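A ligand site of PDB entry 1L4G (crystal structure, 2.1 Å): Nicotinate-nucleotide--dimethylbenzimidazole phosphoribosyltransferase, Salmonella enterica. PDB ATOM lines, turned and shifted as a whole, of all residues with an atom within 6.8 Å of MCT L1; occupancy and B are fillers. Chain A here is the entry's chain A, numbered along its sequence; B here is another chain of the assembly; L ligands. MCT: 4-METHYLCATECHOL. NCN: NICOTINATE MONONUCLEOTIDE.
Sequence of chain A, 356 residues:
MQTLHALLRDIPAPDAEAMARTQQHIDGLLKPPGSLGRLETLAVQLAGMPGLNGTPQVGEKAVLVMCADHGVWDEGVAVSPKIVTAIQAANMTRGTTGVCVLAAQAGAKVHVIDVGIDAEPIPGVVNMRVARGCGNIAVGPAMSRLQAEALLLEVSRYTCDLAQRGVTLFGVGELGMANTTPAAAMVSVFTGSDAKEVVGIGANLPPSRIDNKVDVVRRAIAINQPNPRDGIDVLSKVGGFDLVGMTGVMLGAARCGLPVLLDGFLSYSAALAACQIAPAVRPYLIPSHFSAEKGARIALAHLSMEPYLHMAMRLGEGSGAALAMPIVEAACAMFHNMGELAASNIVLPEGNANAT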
ATOM      1  N   SER A  80       7.792 -22.293 -11.540  1.00  0.00           N
ATOM      2  CA  SER A  80       7.422 -21.271 -12.508  1.00  0.00           C
ATOM      3  C   SER A  80       8.008 -21.659 -13.855  1.00  0.00           C
ATOM      4  O   SER A  80       9.160 -22.092 -13.930  1.00  0.00           O
ATOM      5  CB  SER A  80       7.982 -19.897 -12.126  1.00  0.00           C
ATOM      6  OG  SER A  80       7.561 -19.466 -10.854  1.00  0.00           O
ATOM      7  N   VAL A  84       9.022 -17.373 -17.861  1.00  0.00           N
ATOM      8  CA  VAL A  84       8.541 -16.266 -17.065  1.00  0.00           C
ATOM      9  C   VAL A  84       9.638 -15.221 -16.895  1.00  0.00           C
ATOM     10  O   VAL A  84       9.356 -14.034 -16.817  1.00  0.00           O
ATOM     11  CB  VAL A  84       8.018 -16.745 -15.671  1.00  0.00           C
ATOM     12  CG1 VAL A  84       7.633 -15.556 -14.807  1.00  0.00           C
ATOM     13  CG2 VAL A  84       6.815 -17.641 -15.870  1.00  0.00           C
ATOM     14  N   GLN A  88       8.621 -11.489 -17.869  1.00  0.00           N
ATOM     15  CA  GLN A  88       8.657 -10.512 -16.795  1.00  0.00           C
ATOM     16  C   GLN A  88       9.680  -9.416 -17.079  1.00  0.00           C
ATOM     17  O   GLN A  88       9.456  -8.253 -16.731  1.00  0.00           O
ATOM     18  CB  GLN A  88       9.011 -11.161 -15.464  1.00  0.00           C
ATOM     19  CG  GLN A  88       7.835 -11.423 -14.550  1.00  0.00           C
ATOM     20  CD  GLN A  88       6.970 -10.186 -14.322  1.00  0.00           C
ATOM     21  OE1 GLN A  88       6.220  -9.759 -15.203  1.00  0.00           O
ATOM     22  NE2 GLN A  88       7.071  -9.598 -13.127  1.00  0.00           N
ATOM     23  N   ASN A  91       7.940  -7.051 -19.256  1.00  0.00           N
ATOM     24  CA  ASN A  91       6.998  -6.228 -18.487  1.00  0.00           C
ATOM     25  C   ASN A  91       7.699  -5.118 -17.703  1.00  0.00           C
ATOM     26  O   ASN A  91       7.105  -4.079 -17.409  1.00  0.00           O
ATOM     27  CB  ASN A  91       6.174  -7.088 -17.530  1.00  0.00           C
ATOM     28  CG  ASN A  91       5.192  -7.987 -18.253  1.00  0.00           C
ATOM     29  OD1 ASN A  91       4.599  -7.598 -19.256  1.00  0.00           O
ATOM     30  ND2 ASN A  91       4.993  -9.202 -17.738  1.00  0.00           N
ATOM     31  N   MET A  92       8.961  -5.344 -17.347  1.00  0.00           N
ATOM     32  CA  MET A  92       9.735  -4.343 -16.617  1.00  0.00           C
ATOM     33  C   MET A  92       9.824  -3.053 -17.436  1.00  0.00           C
ATOM     34  O   MET A  92       9.819  -1.956 -16.884  1.00  0.00           O
ATOM     35  CB  MET A  92      11.147  -4.857 -16.360  1.00  0.00           C
ATOM     36  CG  MET A  92      11.240  -6.017 -15.411  1.00  0.00           C
ATOM     37  SD  MET A  92      11.334  -5.491 -13.708  1.00  0.00           S
ATOM     38  CE  MET A  92      11.278  -7.072 -12.879  1.00  0.00           C
ATOM     39  N   THR A  97       5.327  -4.159 -13.455  1.00  0.00           N
ATOM     40  CA  THR A  97       5.781  -5.098 -12.430  1.00  0.00           C
ATOM     41  C   THR A  97       5.796  -4.468 -11.036  1.00  0.00           C
ATOM     42  O   THR A  97       5.702  -3.239 -10.900  1.00  0.00           O
ATOM     43  CB  THR A  97       7.222  -5.589 -12.719  1.00  0.00           C
ATOM     44  OG1 THR A  97       8.143  -4.544 -12.389  1.00  0.00           O
ATOM     45  CG2 THR A  97       7.393  -5.940 -14.201  1.00  0.00           C
ATOM     46  N   GLY A  98       5.955  -5.313 -10.018  1.00  0.00           N
ATOM     47  CA  GLY A  98       6.008  -4.822  -8.657  1.00  0.00           C
ATOM     48  C   GLY A  98       7.075  -3.762  -8.399  1.00  0.00           C
ATOM     49  O   GLY A  98       6.785  -2.714  -7.837  1.00  0.00           O
ATOM     50  N   GLU A 174      16.848  -8.559  -8.730  1.00  0.00           N
ATOM     51  CA  GLU A 174      17.000  -9.609  -9.724  1.00  0.00           C
ATOM     52  C   GLU A 174      15.690 -10.204 -10.229  1.00  0.00           C
ATOM     53  O   GLU A 174      14.614  -9.882  -9.742  1.00  0.00           O
ATOM     54  CB  GLU A 174      17.863 -10.743  -9.157  1.00  0.00           C
ATOM     55  CG  GLU A 174      17.532 -11.143  -7.726  1.00  0.00           C
ATOM     56  CD  GLU A 174      16.071 -11.544  -7.567  1.00  0.00           C
ATOM     57  OE1 GLU A 174      15.652 -12.548  -8.152  1.00  0.00           O
ATOM     58  OE2 GLU A 174      15.339 -10.856  -6.844  1.00  0.00           O
ATOM     59  N   LEU A 175      15.841 -11.092 -11.205  1.00  0.00           N
ATOM     60  CA  LEU A 175      14.732 -11.788 -11.825  1.00  0.00           C
ATOM     61  C   LEU A 175      15.296 -13.028 -12.518  1.00  0.00           C
ATOM     62  O   LEU A 175      16.117 -12.922 -13.433  1.00  0.00           O
ATOM     63  CB  LEU A 175      14.054 -10.876 -12.847  1.00  0.00           C
ATOM     64  CG  LEU A 175      12.825 -11.440 -13.560  1.00  0.00           C
ATOM     65  CD1 LEU A 175      11.730 -11.729 -12.529  1.00  0.00           C
ATOM     66  CD2 LEU A 175      12.333 -10.430 -14.601  1.00  0.00           C
ATOM     67  N   GLY A 176      14.870 -14.207 -12.083  1.00  0.00           N
ATOM     68  CA  GLY A 176      15.373 -15.439 -12.687  1.00  0.00           C
ATOM     69  C   GLY A 176      14.811 -16.679 -12.017  1.00  0.00           C
ATOM     70  O   GLY A 176      15.176 -17.003 -10.887  1.00  0.00           O
ATOM     71  N   MET A 177      13.937 -17.400 -12.734  1.00  0.00           N
ATOM     72  CA  MET A 177      13.328 -18.616 -12.211  1.00  0.00           C
ATOM     73  C   MET A 177      14.399 -19.605 -11.737  1.00  0.00           C
ATOM     74  O   MET A 177      15.364 -19.885 -12.457  1.00  0.00           O
ATOM     75  CB  MET A 177      12.445 -19.284 -13.287  1.00  0.00           C
ATOM     76  CG  MET A 177      11.448 -18.365 -13.973  1.00  0.00           C
ATOM     77  SD  MET A 177      10.346 -17.508 -12.804  1.00  0.00           S
ATOM     78  CE  MET A 177      11.161 -15.898 -12.689  1.00  0.00           C
ATOM     79  N   ASN A 179      16.424 -19.169  -9.085  1.00  0.00           N
ATOM     80  CA  ASN A 179      17.622 -18.585  -8.451  1.00  0.00           C
ATOM     81  C   ASN A 179      17.759 -18.706  -6.923  1.00  0.00           C
ATOM     82  O   ASN A 179      18.830 -18.444  -6.394  1.00  0.00           O
ATOM     83  CB  ASN A 179      17.846 -17.118  -8.913  1.00  0.00           C
ATOM     84  CG  ASN A 179      16.784 -16.150  -8.440  1.00  0.00           C
ATOM     85  OD1 ASN A 179      15.928 -16.477  -7.618  1.00  0.00           O
ATOM     86  ND2 ASN A 179      16.861 -14.931  -8.946  1.00  0.00           N
ATOM     87  N   ALA A 203       9.623 -19.277  -5.020  1.00  0.00           N
ATOM     88  CA  ALA A 203       8.357 -18.798  -5.564  1.00  0.00           C
ATOM     89  C   ALA A 203       7.281 -19.880  -5.485  1.00  0.00           C
ATOM     90  O   ALA A 203       6.947 -20.537  -6.472  1.00  0.00           O
ATOM     91  CB  ALA A 203       8.547 -18.343  -7.015  1.00  0.00           C
ATOM     92  N   ARG A 314       8.577 -11.667  -0.524  1.00  0.00           N
ATOM     93  CA  ARG A 314       9.443 -12.656  -1.168  1.00  0.00           C
ATOM     94  C   ARG A 314       9.232 -12.630  -2.676  1.00  0.00           C
ATOM     95  O   ARG A 314       9.219 -13.664  -3.336  1.00  0.00           O
ATOM     96  CB  ARG A 314       9.129 -14.054  -0.599  1.00  0.00           C
ATOM     97  CG  ARG A 314       7.646 -14.416  -0.607  1.00  0.00           C
ATOM     98  CD  ARG A 314       7.362 -15.726   0.135  1.00  0.00           C
ATOM     99  NE  ARG A 314       5.930 -15.986   0.310  1.00  0.00           N
ATOM    100  CZ  ARG A 314       5.107 -16.384  -0.655  1.00  0.00           C
ATOM    101  NH1 ARG A 314       5.550 -16.576  -1.888  1.00  0.00           N
ATOM    102  NH2 ARG A 314       3.829 -16.597  -0.392  1.00  0.00           N
ATOM    103  N   LEU A 315       9.064 -11.421  -3.216  1.00  0.00           N
ATOM    104  CA  LEU A 315       8.857 -11.244  -4.643  1.00  0.00           C
ATOM    105  C   LEU A 315      10.146 -11.108  -5.455  1.00  0.00           C
ATOM    106  O   LEU A 315      10.296 -11.707  -6.515  1.00  0.00           O
ATOM    107  CB  LEU A 315       7.998 -10.011  -4.892  1.00  0.00           C
ATOM    108  CG  LEU A 315       7.877  -9.561  -6.353  1.00  0.00           C
ATOM    109  CD1 LEU A 315       7.120 -10.605  -7.184  1.00  0.00           C
ATOM    110  CD2 LEU A 315       7.146  -8.232  -6.401  1.00  0.00           C
ATOM    111  N   GLY A 316      11.078 -10.294  -4.944  1.00  0.00           N
ATOM    112  CA  GLY A 316      12.317 -10.052  -5.649  1.00  0.00           C
ATOM    113  C   GLY A 316      12.138  -8.781  -6.475  1.00  0.00           C
ATOM    114  O   GLY A 316      11.343  -7.915  -6.104  1.00  0.00           O
ATOM    115  N   GLU A 317      12.867  -8.699  -7.594  1.00  0.00           N
ATOM    116  CA  GLU A 317      12.847  -7.540  -8.503  1.00  0.00           C
ATOM    117  C   GLU A 317      13.460  -6.286  -7.885  1.00  0.00           C
ATOM    118  O   GLU A 317      13.624  -5.266  -8.572  1.00  0.00           O
ATOM    119  CB  GLU A 317      11.402  -7.222  -8.917  1.00  0.00           C
ATOM    120  CG  GLU A 317      10.587  -8.414  -9.342  1.00  0.00           C
ATOM    121  CD  GLU A 317       9.238  -8.021  -9.899  1.00  0.00           C
ATOM    122  OE1 GLU A 317       8.825  -6.866  -9.695  1.00  0.00           O
ATOM    123  OE2 GLU A 317       8.582  -8.855 -10.546  1.00  0.00           O
ATOM    124  N   LEU B  29      -2.518 -10.479  -9.770  1.00  0.00           N
ATOM    125  CA  LEU B  29      -1.478  -9.538 -10.176  1.00  0.00           C
ATOM    126  C   LEU B  29      -0.207 -10.234 -10.641  1.00  0.00           C
ATOM    127  O   LEU B  29       0.055 -11.386 -10.296  1.00  0.00           O
ATOM    128  CB  LEU B  29      -1.175  -8.575  -9.024  1.00  0.00           C
ATOM    129  CG  LEU B  29      -2.350  -7.700  -8.565  1.00  0.00           C
ATOM    130  CD1 LEU B  29      -1.902  -6.811  -7.418  1.00  0.00           C
ATOM    131  CD2 LEU B  29      -2.867  -6.859  -9.735  1.00  0.00           C
ATOM    132  N   LEU B  30       0.595  -9.521 -11.418  1.00  0.00           N
ATOM    133  CA  LEU B  30       1.833 -10.047 -11.988  1.00  0.00           C
ATOM    134  C   LEU B  30       2.862 -10.444 -10.934  1.00  0.00           C
ATOM    135  O   LEU B  30       3.889  -9.783 -10.771  1.00  0.00           O
ATOM    136  CB  LEU B  30       2.415  -9.000 -12.938  1.00  0.00           C
ATOM    137  CG  LEU B  30       2.996  -9.417 -14.271  1.00  0.00           C
ATOM    138  CD1 LEU B  30       2.216 -10.551 -14.920  1.00  0.00           C
ATOM    139  CD2 LEU B  30       2.989  -8.181 -15.156  1.00  0.00           C
ATOM    140  N   LYS B  31       2.593 -11.539 -10.226  1.00  0.00           N
ATOM    141  CA  LYS B  31       3.508 -12.002  -9.184  1.00  0.00           C
ATOM    142  C   LYS B  31       3.048 -13.332  -8.618  1.00  0.00           C
ATOM    143  O   LYS B  31       1.892 -13.728  -8.762  1.00  0.00           O
ATOM    144  CB  LYS B  31       3.543 -10.994  -8.028  1.00  0.00           C
ATOM    145  CG  LYS B  31       2.167 -10.818  -7.358  1.00  0.00           C
ATOM    146  CD  LYS B  31       2.228  -9.957  -6.114  1.00  0.00           C
ATOM    147  CE  LYS B  31       0.842  -9.651  -5.587  1.00  0.00           C
ATOM    148  NZ  LYS B  31       0.033 -10.873  -5.372  1.00  0.00           N
ATOM    149  N   PRO B  32       3.978 -14.059  -7.969  1.00  0.00           N
ATOM    150  CA  PRO B  32       3.595 -15.347  -7.376  1.00  0.00           C
ATOM    151  C   PRO B  32       2.573 -15.014  -6.296  1.00  0.00           C
ATOM    152  O   PRO B  32       2.732 -14.033  -5.552  1.00  0.00           O
ATOM    153  CB  PRO B  32       4.907 -15.843  -6.772  1.00  0.00           C
ATOM    154  CG  PRO B  32       5.931 -15.285  -7.717  1.00  0.00           C
ATOM    155  CD  PRO B  32       5.440 -13.882  -7.952  1.00  0.00           C
ATOM    156  N   SER B  35       3.279 -13.439  -2.724  1.00  0.00           N
ATOM    157  CA  SER B  35       4.676 -13.003  -2.682  1.00  0.00           C
ATOM    158  C   SER B  35       4.899 -11.621  -2.082  1.00  0.00           C
ATOM    159  O   SER B  35       5.980 -11.335  -1.590  1.00  0.00           O
ATOM    160  CB  SER B  35       5.301 -13.074  -4.077  1.00  0.00           C
ATOM    161  OG  SER B  35       4.585 -12.288  -5.017  1.00  0.00           O
ATOM    162  N   LEU B 341      -1.356 -11.317 -14.385  1.00  0.00           N
ATOM    163  CA  LEU B 341      -0.814 -12.551 -14.956  1.00  0.00           C
ATOM    164  C   LEU B 341      -1.511 -12.981 -16.246  1.00  0.00           C
ATOM    165  O   LEU B 341      -0.854 -13.262 -17.254  1.00  0.00           O
ATOM    166  CB  LEU B 341      -0.909 -13.678 -13.928  1.00  0.00           C
ATOM    167  CG  LEU B 341      -0.053 -13.582 -12.669  1.00  0.00           C
ATOM    168  CD1 LEU B 341      -0.519 -14.583 -11.621  1.00  0.00           C
ATOM    169  CD2 LEU B 341       1.400 -13.848 -13.043  1.00  0.00           C
ATOM    170  N   ILE B 346       0.660 -15.661 -18.359  1.00  0.00           N
ATOM    171  CA  ILE B 346       1.500 -16.381 -17.410  1.00  0.00           C
ATOM    172  C   ILE B 346       0.608 -17.231 -16.516  1.00  0.00           C
ATOM    173  O   ILE B 346      -0.375 -16.735 -15.961  1.00  0.00           O
ATOM    174  CB  ILE B 346       2.331 -15.417 -16.536  1.00  0.00           C
ATOM    175  CG1 ILE B 346       3.257 -14.574 -17.417  1.00  0.00           C
ATOM    176  CG2 ILE B 346       3.139 -16.192 -15.516  1.00  0.00           C
ATOM    177  CD1 ILE B 346       4.005 -13.483 -16.653  1.00  0.00           C
ATOM    178  N   LEU B 348       0.802 -19.680 -13.233  1.00  0.00           N
ATOM    179  CA  LEU B 348       1.566 -20.195 -12.098  1.00  0.00           C
ATOM    180  C   LEU B 348       0.668 -21.032 -11.187  1.00  0.00           C
ATOM    181  O   LEU B 348      -0.507 -20.726 -11.019  1.00  0.00           O
ATOM    182  CB  LEU B 348       2.176 -19.045 -11.303  1.00  0.00           C
ATOM    183  CG  LEU B 348       3.122 -18.130 -12.090  1.00  0.00           C
ATOM    184  CD1 LEU B 348       3.380 -16.851 -11.323  1.00  0.00           C
ATOM    185  CD2 LEU B 348       4.406 -18.865 -12.384  1.00  0.00           C
HETATM  186  C1  MCT L   1       6.598 -13.454 -11.568  1.00  0.00           C
HETATM  187  C2  MCT L   1       7.254 -12.304 -11.085  1.00  0.00           C
HETATM  188  C3  MCT L   1       8.362 -12.427 -10.296  1.00  0.00           C
HETATM  189  O3  MCT L   1       9.053 -11.250  -9.790  1.00  0.00           O
HETATM  190  C4  MCT L   1       8.850 -13.715  -9.973  1.00  0.00           C
HETATM  191  O4  MCT L   1      10.005 -13.769  -9.149  1.00  0.00           O
HETATM  192  C5  MCT L   1       8.230 -14.866 -10.437  1.00  0.00           C
HETATM  193  C6  MCT L   1       7.099 -14.757 -11.235  1.00  0.00           C
HETATM  194  C   MCT L   1       5.366 -13.342 -12.443  1.00  0.00           C
HETATM  195  P   NCN L   2      12.426 -19.860  -7.351  1.00  0.00           P
HETATM  196  O1P NCN L   2      13.771 -20.343  -6.944  1.00  0.00           O
HETATM  197  O2P NCN L   2      11.380 -20.704  -6.703  1.00  0.00           O
HETATM  198  O3P NCN L   2      12.251 -19.939  -8.977  1.00  0.00           O
HETATM  199  O5' NCN L   2      12.223 -18.365  -6.872  1.00  0.00           O
HETATM  200  C5' NCN L   2      13.121 -17.338  -7.340  1.00  0.00           C
HETATM  201  C4' NCN L   2      12.376 -16.349  -8.034  1.00  0.00           C
HETATM  202  O4' NCN L   2      11.321 -15.817  -7.181  1.00  0.00           O
HETATM  203  C3' NCN L   2      13.142 -15.158  -8.554  1.00  0.00           C
HETATM  204  O3' NCN L   2      12.660 -14.691  -9.842  1.00  0.00           O
HETATM  205  C2' NCN L   2      12.958 -14.126  -7.399  1.00  0.00           C
HETATM  206  O2' NCN L   2      12.810 -12.801  -7.966  1.00  0.00           O
HETATM  207  C1' NCN L   2      11.732 -14.615  -6.596  1.00  0.00           C
HETATM  208  N1  NCN L   2      11.914 -14.810  -5.105  1.00  0.00           N
HETATM  209  C6  NCN L   2      11.466 -15.999  -4.424  1.00  0.00           C
HETATM  210  C5  NCN L   2      11.715 -15.994  -3.048  1.00  0.00           C
HETATM  211  C4  NCN L   2      12.349 -14.955  -2.295  1.00  0.00           C
HETATM  212  C3  NCN L   2      12.742 -13.807  -3.118  1.00  0.00           C
HETATM  213  C2  NCN L   2      12.534 -13.741  -4.486  1.00  0.00           C
HETATM  214  C7  NCN L   2      13.390 -12.787  -2.188  1.00  0.00           C
HETATM  215  O7  NCN L   2      13.566 -12.863  -0.995  1.00  0.00           O
HETATM  216  O8  NCN L   2      13.749 -11.739  -2.914  1.00  0.00           O
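The side-chain carboxylate (OE2) of Glu 317 is in hydrogen-bond range of an oxygen (O3) of MCT L1.
The backbone carbonyl oxygen of Leu 315 sits at hydrogen-bond distance from an oxygen (O4) of MCT L1.
The backbone carbonyl oxygen of Leu 315 sits at hydrogen-bond distance from an oxygen (O2') of NCN L2 (3.1 Å).
The backbone NH (N) of Ala 203 lies within hydrogen-bond range of an oxygen (O2P) of NCN L2, at 2.8 Å.
An oxygen (O3') of NCN L2 sits at hydrogen-bond distance from the backbone NH of Gly 176, 3.2 Å away.
The side-chain carboxylate of Glu 174 sits at hydrogen-bond distance from an oxygen (O2') of NCN L2.
An oxygen (O4) of MCT L1 is in hydrogen-bond range of an oxygen (O3') of NCN L2 (2.9 Å).
OE2 of Glu 317 lies within hydrogen-bond range of NE2 of Gln 88, 3.1 Å away.
N of Glu 317 is in hydrogen-bond range of O of Glu 174 (3.0 Å).
The side-chain carboxylate (OE1) of Glu 317 lies within hydrogen-bond range of the backbone NH (N) of Gly 98 (3.3 Å).
O of Ser 35 of chain B sits at hydrogen-bond distance from N of Leu 315 (3.5 Å).
The side-chain amide oxygen (OE1) of Gln 88 sits at hydrogen-bond distance from the side-chain amide nitrogen (ND2) of Asn 91, at 2.9 Å.
The backbone carbonyl oxygen (O) of Pro 32 of chain B sits at hydrogen-bond distance from the side-chain hydroxyl (OG) of Ser 35 of chain B (2.6 Å).
Val 84 touches MCT L1 (CG1 to C6, 3.7 Å).
Gln 88 touches MCT L1.
CD1 of Leu 175 touches O3 of MCT L1, at 3.9 Å.
Met 177 touches MCT L1.
Lys 31 of chain B touches MCT L1.
CG of Pro 32 of chain B touches C5 of MCT L1 (3.6 Å).
Hydrophobic or aromatic side chains that line MCT L1: Val 84, Leu 175, Met 177, Leu 315 and Pro 32 of chain B.
Of the 25 residues printed, 8 come within 4 Å of MCT L1.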
